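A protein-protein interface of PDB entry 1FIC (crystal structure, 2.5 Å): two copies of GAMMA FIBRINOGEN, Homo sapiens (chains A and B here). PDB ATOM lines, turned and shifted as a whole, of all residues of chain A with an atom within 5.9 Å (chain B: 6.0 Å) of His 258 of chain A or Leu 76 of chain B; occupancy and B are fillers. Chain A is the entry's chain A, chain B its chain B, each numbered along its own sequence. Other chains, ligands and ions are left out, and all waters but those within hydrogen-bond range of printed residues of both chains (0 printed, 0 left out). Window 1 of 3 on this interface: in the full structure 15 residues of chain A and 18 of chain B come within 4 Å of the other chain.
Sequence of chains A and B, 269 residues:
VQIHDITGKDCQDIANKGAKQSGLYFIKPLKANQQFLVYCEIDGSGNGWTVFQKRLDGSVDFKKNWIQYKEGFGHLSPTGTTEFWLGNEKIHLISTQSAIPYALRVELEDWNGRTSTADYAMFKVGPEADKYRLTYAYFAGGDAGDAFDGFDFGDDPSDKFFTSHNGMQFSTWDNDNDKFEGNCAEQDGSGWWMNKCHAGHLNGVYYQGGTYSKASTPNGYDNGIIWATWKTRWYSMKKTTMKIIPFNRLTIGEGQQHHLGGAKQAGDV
No position is printed for both chains. Of the 12 pairs that touch across the chains among the printed residues, none has its exchanged pair printed and touching as well.
The backbone NH of Leu 76 of chain B sits at hydrogen-bond distance from the backbone carbonyl oxygen of His 258 of chain A (2.6 Å). ND1 of His 259 of chain A lies within hydrogen-bond range of ND1 of His 75 of chain B, 2.8 Å away. The backbone NH (N) of Leu 260 of chain A lies within hydrogen-bond range of the backbone carbonyl oxygen (O) of Gly 74 of chain B (2.8 Å).
CG of Gln 2 of chain B touches OE1 of Gln 256 of chain A, at 3.1 Å. Gln 256 of chain A touches Ser 77 of chain B. O of Gln 256 of chain A touches CD of Pro 78 of chain B, at 3.4 Å. CA of Gln 257 of chain A touches O of Leu 76 of chain B (3.4 Å). Gln 257 of chain A touches Thr 82 of chain B. CD1 of Leu 37 of chain B touches ND1 of His 258 of chain A, at 3.7 Å. CA of His 75 of chain B touches O of His 258 of chain A, at 3.1 Å. His 259 of chain A touches Gly 74 of chain B (CA to O, 3.7 Å). CD2 of Leu 260 of chain A touches CG of Leu 76 of chain B (3.6 Å).
The backbone carbonyl oxygen (O) of Glu 83 of chain B is in hydrogen-bond range of the backbone NH (N) of His 75 of chain B (3.1 Å). The side-chain hydroxyl (OG) of Ser 77 of chain B sits at hydrogen-bond distance from the side-chain hydroxyl (OG1) of Thr 82 of chain B, 2.8 Å away.
Printed residues of chain A that touch a printed residue of chain B: Gln 256, Gln 257, His 258, His 259 and Leu 260. Hydrophobic or aromatic side chains of chain A within 4 Å of the printed part of chain B: His 258, His 259 and Leu 260. Among the printed residues, no Asp or Glu carboxylate lies within 4 Å of a Lys or Arg side-chain nitrogen of the other chain.
His 258 of chain A touches three residues of chain B. Leu 76 of chain B touches three residues of chain A. Of the printed residues of chain B, Gln 257 of chain A touches Leu 76 (3.4 Å) and Thr 82 (3.3 Å). Of the printed residues of chain B, Gln 256 of chain A touches Gln 2, Ser 77 and Pro 78. Printed residues of chain B within 4 Å of His 259 of chain A: Gly 74 and His 75. Printed residues of chain B within 4 Å of Leu 260 of chain A: Gly 74 (2.8 Å) and Leu 76 (3.6 Å). Val 38 of chain B touches none of the printed residues of chain A. Tyr 39 of chain B touches none of the printed residues of chain A. The nearest residue of chain A that does not touch Leu 76 of chain B is Gln 256 of chain A (4.6 Å).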
ATOM      1  N   GLN A 256       8.577 -28.301   4.477  1.00  0.00           N
ATOM      2  CA  GLN A 256       8.742 -28.258   5.917  1.00  0.00           C
ATOM      3  C   GLN A 256      10.032 -27.546   6.287  1.00  0.00           C
ATOM      4  O   GLN A 256      10.793 -28.010   7.122  1.00  0.00           O
ATOM      5  CB  GLN A 256       8.708 -29.674   6.490  1.00  0.00           C
ATOM      6  CG  GLN A 256       8.129 -29.766   7.909  1.00  0.00           C
ATOM      7  CD  GLN A 256       6.698 -29.227   8.012  1.00  0.00           C
ATOM      8  OE1 GLN A 256       6.352 -28.530   8.979  1.00  0.00           O
ATOM      9  NE2 GLN A 256       5.863 -29.553   7.022  1.00  0.00           N
ATOM     10  N   GLN A 257      10.280 -26.418   5.634  1.00  0.00           N
ATOM     11  CA  GLN A 257      11.467 -25.611   5.874  1.00  0.00           C
ATOM     12  C   GLN A 257      11.092 -24.158   5.824  1.00  0.00           C
ATOM     13  O   GLN A 257      10.225 -23.753   5.053  1.00  0.00           O
ATOM     14  CB  GLN A 257      12.522 -25.841   4.795  1.00  0.00           C
ATOM     15  CG  GLN A 257      13.164 -27.198   4.830  1.00  0.00           C
ATOM     16  CD  GLN A 257      14.209 -27.367   3.756  1.00  0.00           C
ATOM     17  OE1 GLN A 257      14.372 -26.511   2.880  1.00  0.00           O
ATOM     18  NE2 GLN A 257      14.945 -28.468   3.826  1.00  0.00           N
ATOM     19  N   HIS A 258      11.770 -23.368   6.635  1.00  0.00           N
ATOM     20  CA  HIS A 258      11.546 -21.943   6.673  1.00  0.00           C
ATOM     21  C   HIS A 258      12.834 -21.324   6.146  1.00  0.00           C
ATOM     22  O   HIS A 258      13.907 -21.491   6.729  1.00  0.00           O
ATOM     23  CB  HIS A 258      11.247 -21.478   8.094  1.00  0.00           C
ATOM     24  CG  HIS A 258      11.074 -19.995   8.211  1.00  0.00           C
ATOM     25  ND1 HIS A 258      12.015 -19.181   8.795  1.00  0.00           N
ATOM     26  CD2 HIS A 258      10.085 -19.180   7.769  1.00  0.00           C
ATOM     27  CE1 HIS A 258      11.623 -17.925   8.708  1.00  0.00           C
ATOM     28  NE2 HIS A 258      10.455 -17.897   8.090  1.00  0.00           N
ATOM     29  N   HIS A 259      12.733 -20.654   5.006  1.00  0.00           N
ATOM     30  CA  HIS A 259      13.903 -20.053   4.391  1.00  0.00           C
ATOM     31  C   HIS A 259      14.214 -18.713   5.021  1.00  0.00           C
ATOM     32  O   HIS A 259      13.327 -17.876   5.172  1.00  0.00           O
ATOM     33  CB  HIS A 259      13.702 -19.901   2.878  1.00  0.00           C
ATOM     34  CG  HIS A 259      13.222 -21.153   2.205  1.00  0.00           C
ATOM     35  ND1 HIS A 259      13.806 -22.386   2.412  1.00  0.00           N
ATOM     36  CD2 HIS A 259      12.198 -21.363   1.343  1.00  0.00           C
ATOM     37  CE1 HIS A 259      13.162 -23.298   1.705  1.00  0.00           C
ATOM     38  NE2 HIS A 259      12.183 -22.704   1.050  1.00  0.00           N
ATOM     39  N   LEU A 260      15.453 -18.562   5.472  1.00  0.00           N
ATOM     40  CA  LEU A 260      15.907 -17.319   6.069  1.00  0.00           C
ATOM     41  C   LEU A 260      16.452 -16.482   4.925  1.00  0.00           C
ATOM     42  O   LEU A 260      16.401 -15.246   4.954  1.00  0.00           O
ATOM     43  CB  LEU A 260      17.019 -17.581   7.082  1.00  0.00           C
ATOM     44  CG  LEU A 260      16.764 -18.510   8.252  1.00  0.00           C
ATOM     45  CD1 LEU A 260      17.920 -18.389   9.169  1.00  0.00           C
ATOM     46  CD2 LEU A 260      15.505 -18.124   9.002  1.00  0.00           C
ATOM     47  N   GLN B   2       3.822 -26.732  13.258  1.00  0.00           N
ATOM     48  CA  GLN B   2       5.061 -26.561  12.496  1.00  0.00           C
ATOM     49  C   GLN B   2       5.884 -25.525  13.267  1.00  0.00           C
ATOM     50  O   GLN B   2       7.115 -25.529  13.249  1.00  0.00           O
ATOM     51  CB  GLN B   2       4.738 -26.055  11.078  1.00  0.00           C
ATOM     52  CG  GLN B   2       5.944 -25.763  10.211  1.00  0.00           C
ATOM     53  CD  GLN B   2       5.567 -25.269   8.837  1.00  0.00           C
ATOM     54  OE1 GLN B   2       4.419 -25.411   8.410  1.00  0.00           O
ATOM     55  NE2 GLN B   2       6.538 -24.690   8.124  1.00  0.00           N
ATOM     56  N   ILE B   3       5.180 -24.639  13.955  1.00  0.00           N
ATOM     57  CA  ILE B   3       5.802 -23.614  14.756  1.00  0.00           C
ATOM     58  C   ILE B   3       5.111 -23.752  16.104  1.00  0.00           C
ATOM     59  O   ILE B   3       3.888 -23.887  16.168  1.00  0.00           O
ATOM     60  CB  ILE B   3       5.594 -22.240  14.121  1.00  0.00           C
ATOM     61  CG1 ILE B   3       6.486 -22.138  12.882  1.00  0.00           C
ATOM     62  CG2 ILE B   3       5.901 -21.130  15.107  1.00  0.00           C
ATOM     63  CD1 ILE B   3       6.571 -20.761  12.292  1.00  0.00           C
ATOM     64  N   LEU B  24      10.773 -25.243  15.937  1.00  0.00           N
ATOM     65  CA  LEU B  24      10.792 -23.799  15.711  1.00  0.00           C
ATOM     66  C   LEU B  24       9.868 -23.054  16.686  1.00  0.00           C
ATOM     67  O   LEU B  24       8.725 -23.466  16.922  1.00  0.00           O
ATOM     68  CB  LEU B  24      10.392 -23.501  14.267  1.00  0.00           C
ATOM     69  CG  LEU B  24      11.080 -24.350  13.183  1.00  0.00           C
ATOM     70  CD1 LEU B  24      10.652 -23.877  11.812  1.00  0.00           C
ATOM     71  CD2 LEU B  24      12.594 -24.268  13.312  1.00  0.00           C
ATOM     72  N   LEU B  37      11.847 -16.246  14.267  1.00  0.00           N
ATOM     73  CA  LEU B  37      11.864 -17.679  14.503  1.00  0.00           C
ATOM     74  C   LEU B  37      13.269 -18.136  14.787  1.00  0.00           C
ATOM     75  O   LEU B  37      14.211 -17.594  14.218  1.00  0.00           O
ATOM     76  CB  LEU B  37      11.417 -18.425  13.248  1.00  0.00           C
ATOM     77  CG  LEU B  37       9.992 -18.849  12.951  1.00  0.00           C
ATOM     78  CD1 LEU B  37      10.100 -19.930  11.907  1.00  0.00           C
ATOM     79  CD2 LEU B  37       9.304 -19.408  14.189  1.00  0.00           C
ATOM     80  N   VAL B  38      13.398 -19.177  15.602  1.00  0.00           N
ATOM     81  CA  VAL B  38      14.685 -19.770  15.917  1.00  0.00           C
ATOM     82  C   VAL B  38      14.396 -21.223  16.142  1.00  0.00           C
ATOM     83  O   VAL B  38      13.260 -21.596  16.415  1.00  0.00           O
ATOM     84  CB  VAL B  38      15.281 -19.285  17.228  1.00  0.00           C
ATOM     85  CG1 VAL B  38      15.489 -17.801  17.215  1.00  0.00           C
ATOM     86  CG2 VAL B  38      14.389 -19.703  18.371  1.00  0.00           C
ATOM     87  N   TYR B  39      15.428 -22.043  16.042  1.00  0.00           N
ATOM     88  CA  TYR B  39      15.292 -23.458  16.304  1.00  0.00           C
ATOM     89  C   TYR B  39      15.773 -23.655  17.748  1.00  0.00           C
ATOM     90  O   TYR B  39      16.861 -23.205  18.106  1.00  0.00           O
ATOM     91  CB  TYR B  39      16.173 -24.254  15.345  1.00  0.00           C
ATOM     92  CG  TYR B  39      16.205 -25.729  15.654  1.00  0.00           C
ATOM     93  CD1 TYR B  39      15.239 -26.591  15.144  1.00  0.00           C
ATOM     94  CD2 TYR B  39      17.143 -26.248  16.536  1.00  0.00           C
ATOM     95  CE1 TYR B  39      15.205 -27.929  15.523  1.00  0.00           C
ATOM     96  CE2 TYR B  39      17.116 -27.573  16.916  1.00  0.00           C
ATOM     97  CZ  TYR B  39      16.144 -28.409  16.415  1.00  0.00           C
ATOM     98  OH  TYR B  39      16.116 -29.719  16.848  1.00  0.00           O
ATOM     99  N   VAL B  51      19.839 -22.349  18.842  1.00  0.00           N
ATOM    100  CA  VAL B  51      20.846 -22.670  17.840  1.00  0.00           C
ATOM    101  C   VAL B  51      21.019 -21.558  16.815  1.00  0.00           C
ATOM    102  O   VAL B  51      20.046 -21.071  16.249  1.00  0.00           O
ATOM    103  CB  VAL B  51      20.511 -24.001  17.151  1.00  0.00           C
ATOM    104  CG1 VAL B  51      21.602 -24.371  16.168  1.00  0.00           C
ATOM    105  CG2 VAL B  51      20.366 -25.107  18.192  1.00  0.00           C
ATOM    106  N   GLY B  74      20.035 -19.546   4.780  1.00  0.00           N
ATOM    107  CA  GLY B  74      19.882 -20.967   5.002  1.00  0.00           C
ATOM    108  C   GLY B  74      18.433 -21.232   5.325  1.00  0.00           C
ATOM    109  O   GLY B  74      17.567 -20.407   5.006  1.00  0.00           O
ATOM    110  N   HIS B  75      18.137 -22.353   5.967  1.00  0.00           N
ATOM    111  CA  HIS B  75      16.755 -22.635   6.241  1.00  0.00           C
ATOM    112  C   HIS B  75      16.550 -23.266   7.583  1.00  0.00           C
ATOM    113  O   HIS B  75      17.274 -24.175   7.927  1.00  0.00           O
ATOM    114  CB  HIS B  75      16.221 -23.615   5.201  1.00  0.00           C
ATOM    115  CG  HIS B  75      16.947 -23.581   3.892  1.00  0.00           C
ATOM    116  ND1 HIS B  75      16.554 -22.785   2.835  1.00  0.00           N
ATOM    117  CD2 HIS B  75      18.029 -24.271   3.459  1.00  0.00           C
ATOM    118  CE1 HIS B  75      17.359 -22.991   1.807  1.00  0.00           C
ATOM    119  NE2 HIS B  75      18.265 -23.889   2.160  1.00  0.00           N
ATOM    120  N   LEU B  76      15.558 -22.802   8.328  1.00  0.00           N
ATOM    121  CA  LEU B  76      15.227 -23.410   9.608  1.00  0.00           C
ATOM    122  C   LEU B  76      14.258 -24.587   9.329  1.00  0.00           C
ATOM    123  O   LEU B  76      13.497 -24.559   8.380  1.00  0.00           O
ATOM    124  CB  LEU B  76      14.554 -22.394  10.533  1.00  0.00           C
ATOM    125  CG  LEU B  76      15.299 -21.118  10.935  1.00  0.00           C
ATOM    126  CD1 LEU B  76      14.395 -20.262  11.769  1.00  0.00           C
ATOM    127  CD2 LEU B  76      16.515 -21.466  11.729  1.00  0.00           C
ATOM    128  N   SER B  77      14.287 -25.628  10.142  1.00  0.00           N
ATOM    129  CA  SER B  77      13.401 -26.765   9.940  1.00  0.00           C
ATOM    130  C   SER B  77      13.031 -27.323  11.309  1.00  0.00           C
ATOM    131  O   SER B  77      13.847 -27.296  12.217  1.00  0.00           O
ATOM    132  CB  SER B  77      14.104 -27.820   9.096  1.00  0.00           C
ATOM    133  OG  SER B  77      15.359 -28.166   9.647  1.00  0.00           O
ATOM    134  N   PRO B  78      11.799 -27.848  11.478  1.00  0.00           N
ATOM    135  CA  PRO B  78      11.376 -28.396  12.778  1.00  0.00           C
ATOM    136  C   PRO B  78      12.226 -29.587  13.226  1.00  0.00           C
ATOM    137  O   PRO B  78      12.300 -29.925  14.407  1.00  0.00           O
ATOM    138  CB  PRO B  78       9.928 -28.827  12.518  1.00  0.00           C
ATOM    139  CG  PRO B  78       9.504 -28.001  11.327  1.00  0.00           C
ATOM    140  CD  PRO B  78      10.730 -27.999  10.473  1.00  0.00           C
ATOM    141  N   THR B  82      18.693 -28.839   8.665  1.00  0.00           N
ATOM    142  CA  THR B  82      19.034 -27.945   7.578  1.00  0.00           C
ATOM    143  C   THR B  82      20.178 -27.087   8.068  1.00  0.00           C
ATOM    144  O   THR B  82      20.376 -26.937   9.274  1.00  0.00           O
ATOM    145  CB  THR B  82      17.841 -27.020   7.241  1.00  0.00           C
ATOM    146  OG1 THR B  82      17.299 -26.507   8.460  1.00  0.00           O
ATOM    147  CG2 THR B  82      16.738 -27.780   6.514  1.00  0.00           C
ATOM    148  N   GLU B  83      20.937 -26.549   7.123  1.00  0.00           N
ATOM    149  CA  GLU B  83      22.061 -25.683   7.424  1.00  0.00           C
ATOM    150  C   GLU B  83      21.574 -24.257   7.406  1.00  0.00           C
ATOM    151  O   GLU B  83      20.697 -23.918   6.606  1.00  0.00           O
ATOM    152  CB  GLU B  83      23.141 -25.823   6.359  1.00  0.00           C
ATOM    153  CG  GLU B  83      23.617 -27.215   6.186  1.00  0.00           C
ATOM    154  CD  GLU B  83      24.872 -27.289   5.406  1.00  0.00           C
ATOM    155  OE1 GLU B  83      25.034 -26.497   4.464  1.00  0.00           O
ATOM    156  OE2 GLU B  83      25.717 -28.140   5.732  1.00  0.00           O
ATOM    157  N   PHE B  84      22.192 -23.415   8.232  1.00  0.00           N
ATOM    158  CA  PHE B  84      21.841 -22.004   8.302  1.00  0.00           C
ATOM    159  C   PHE B  84      22.795 -21.193   9.178  1.00  0.00           C
ATOM    160  O   PHE B  84      23.661 -21.735   9.846  1.00  0.00           O
ATOM    161  CB  PHE B  84      20.423 -21.850   8.860  1.00  0.00           C
ATOM    162  CG  PHE B  84      20.302 -22.130  10.352  1.00  0.00           C
ATOM    163  CD1 PHE B  84      20.089 -23.430  10.828  1.00  0.00           C
ATOM    164  CD2 PHE B  84      20.339 -21.084  11.274  1.00  0.00           C
ATOM    165  CE1 PHE B  84      19.911 -23.679  12.179  1.00  0.00           C
ATOM    166  CE2 PHE B  84      20.162 -21.334  12.631  1.00  0.00           C
ATOM    167  CZ  PHE B  84      19.945 -22.639  13.077  1.00  0.00           C
ATOM    168  N   LEU B  86      21.859 -17.935  11.652  1.00  0.00           N
ATOM    169  CA  LEU B  86      20.768 -17.113  12.128  1.00  0.00           C
ATOM    170  C   LEU B  86      20.923 -15.656  11.756  1.00  0.00           C
ATOM    171  O   LEU B  86      19.939 -14.955  11.562  1.00  0.00           O
ATOM    172  CB  LEU B  86      20.637 -17.248  13.644  1.00  0.00           C
ATOM    173  CG  LEU B  86      19.390 -16.674  14.329  1.00  0.00           C
ATOM    174  CD1 LEU B  86      18.148 -17.284  13.711  1.00  0.00           C
ATOM    175  CD2 LEU B  86      19.421 -16.984  15.835  1.00  0.00           C
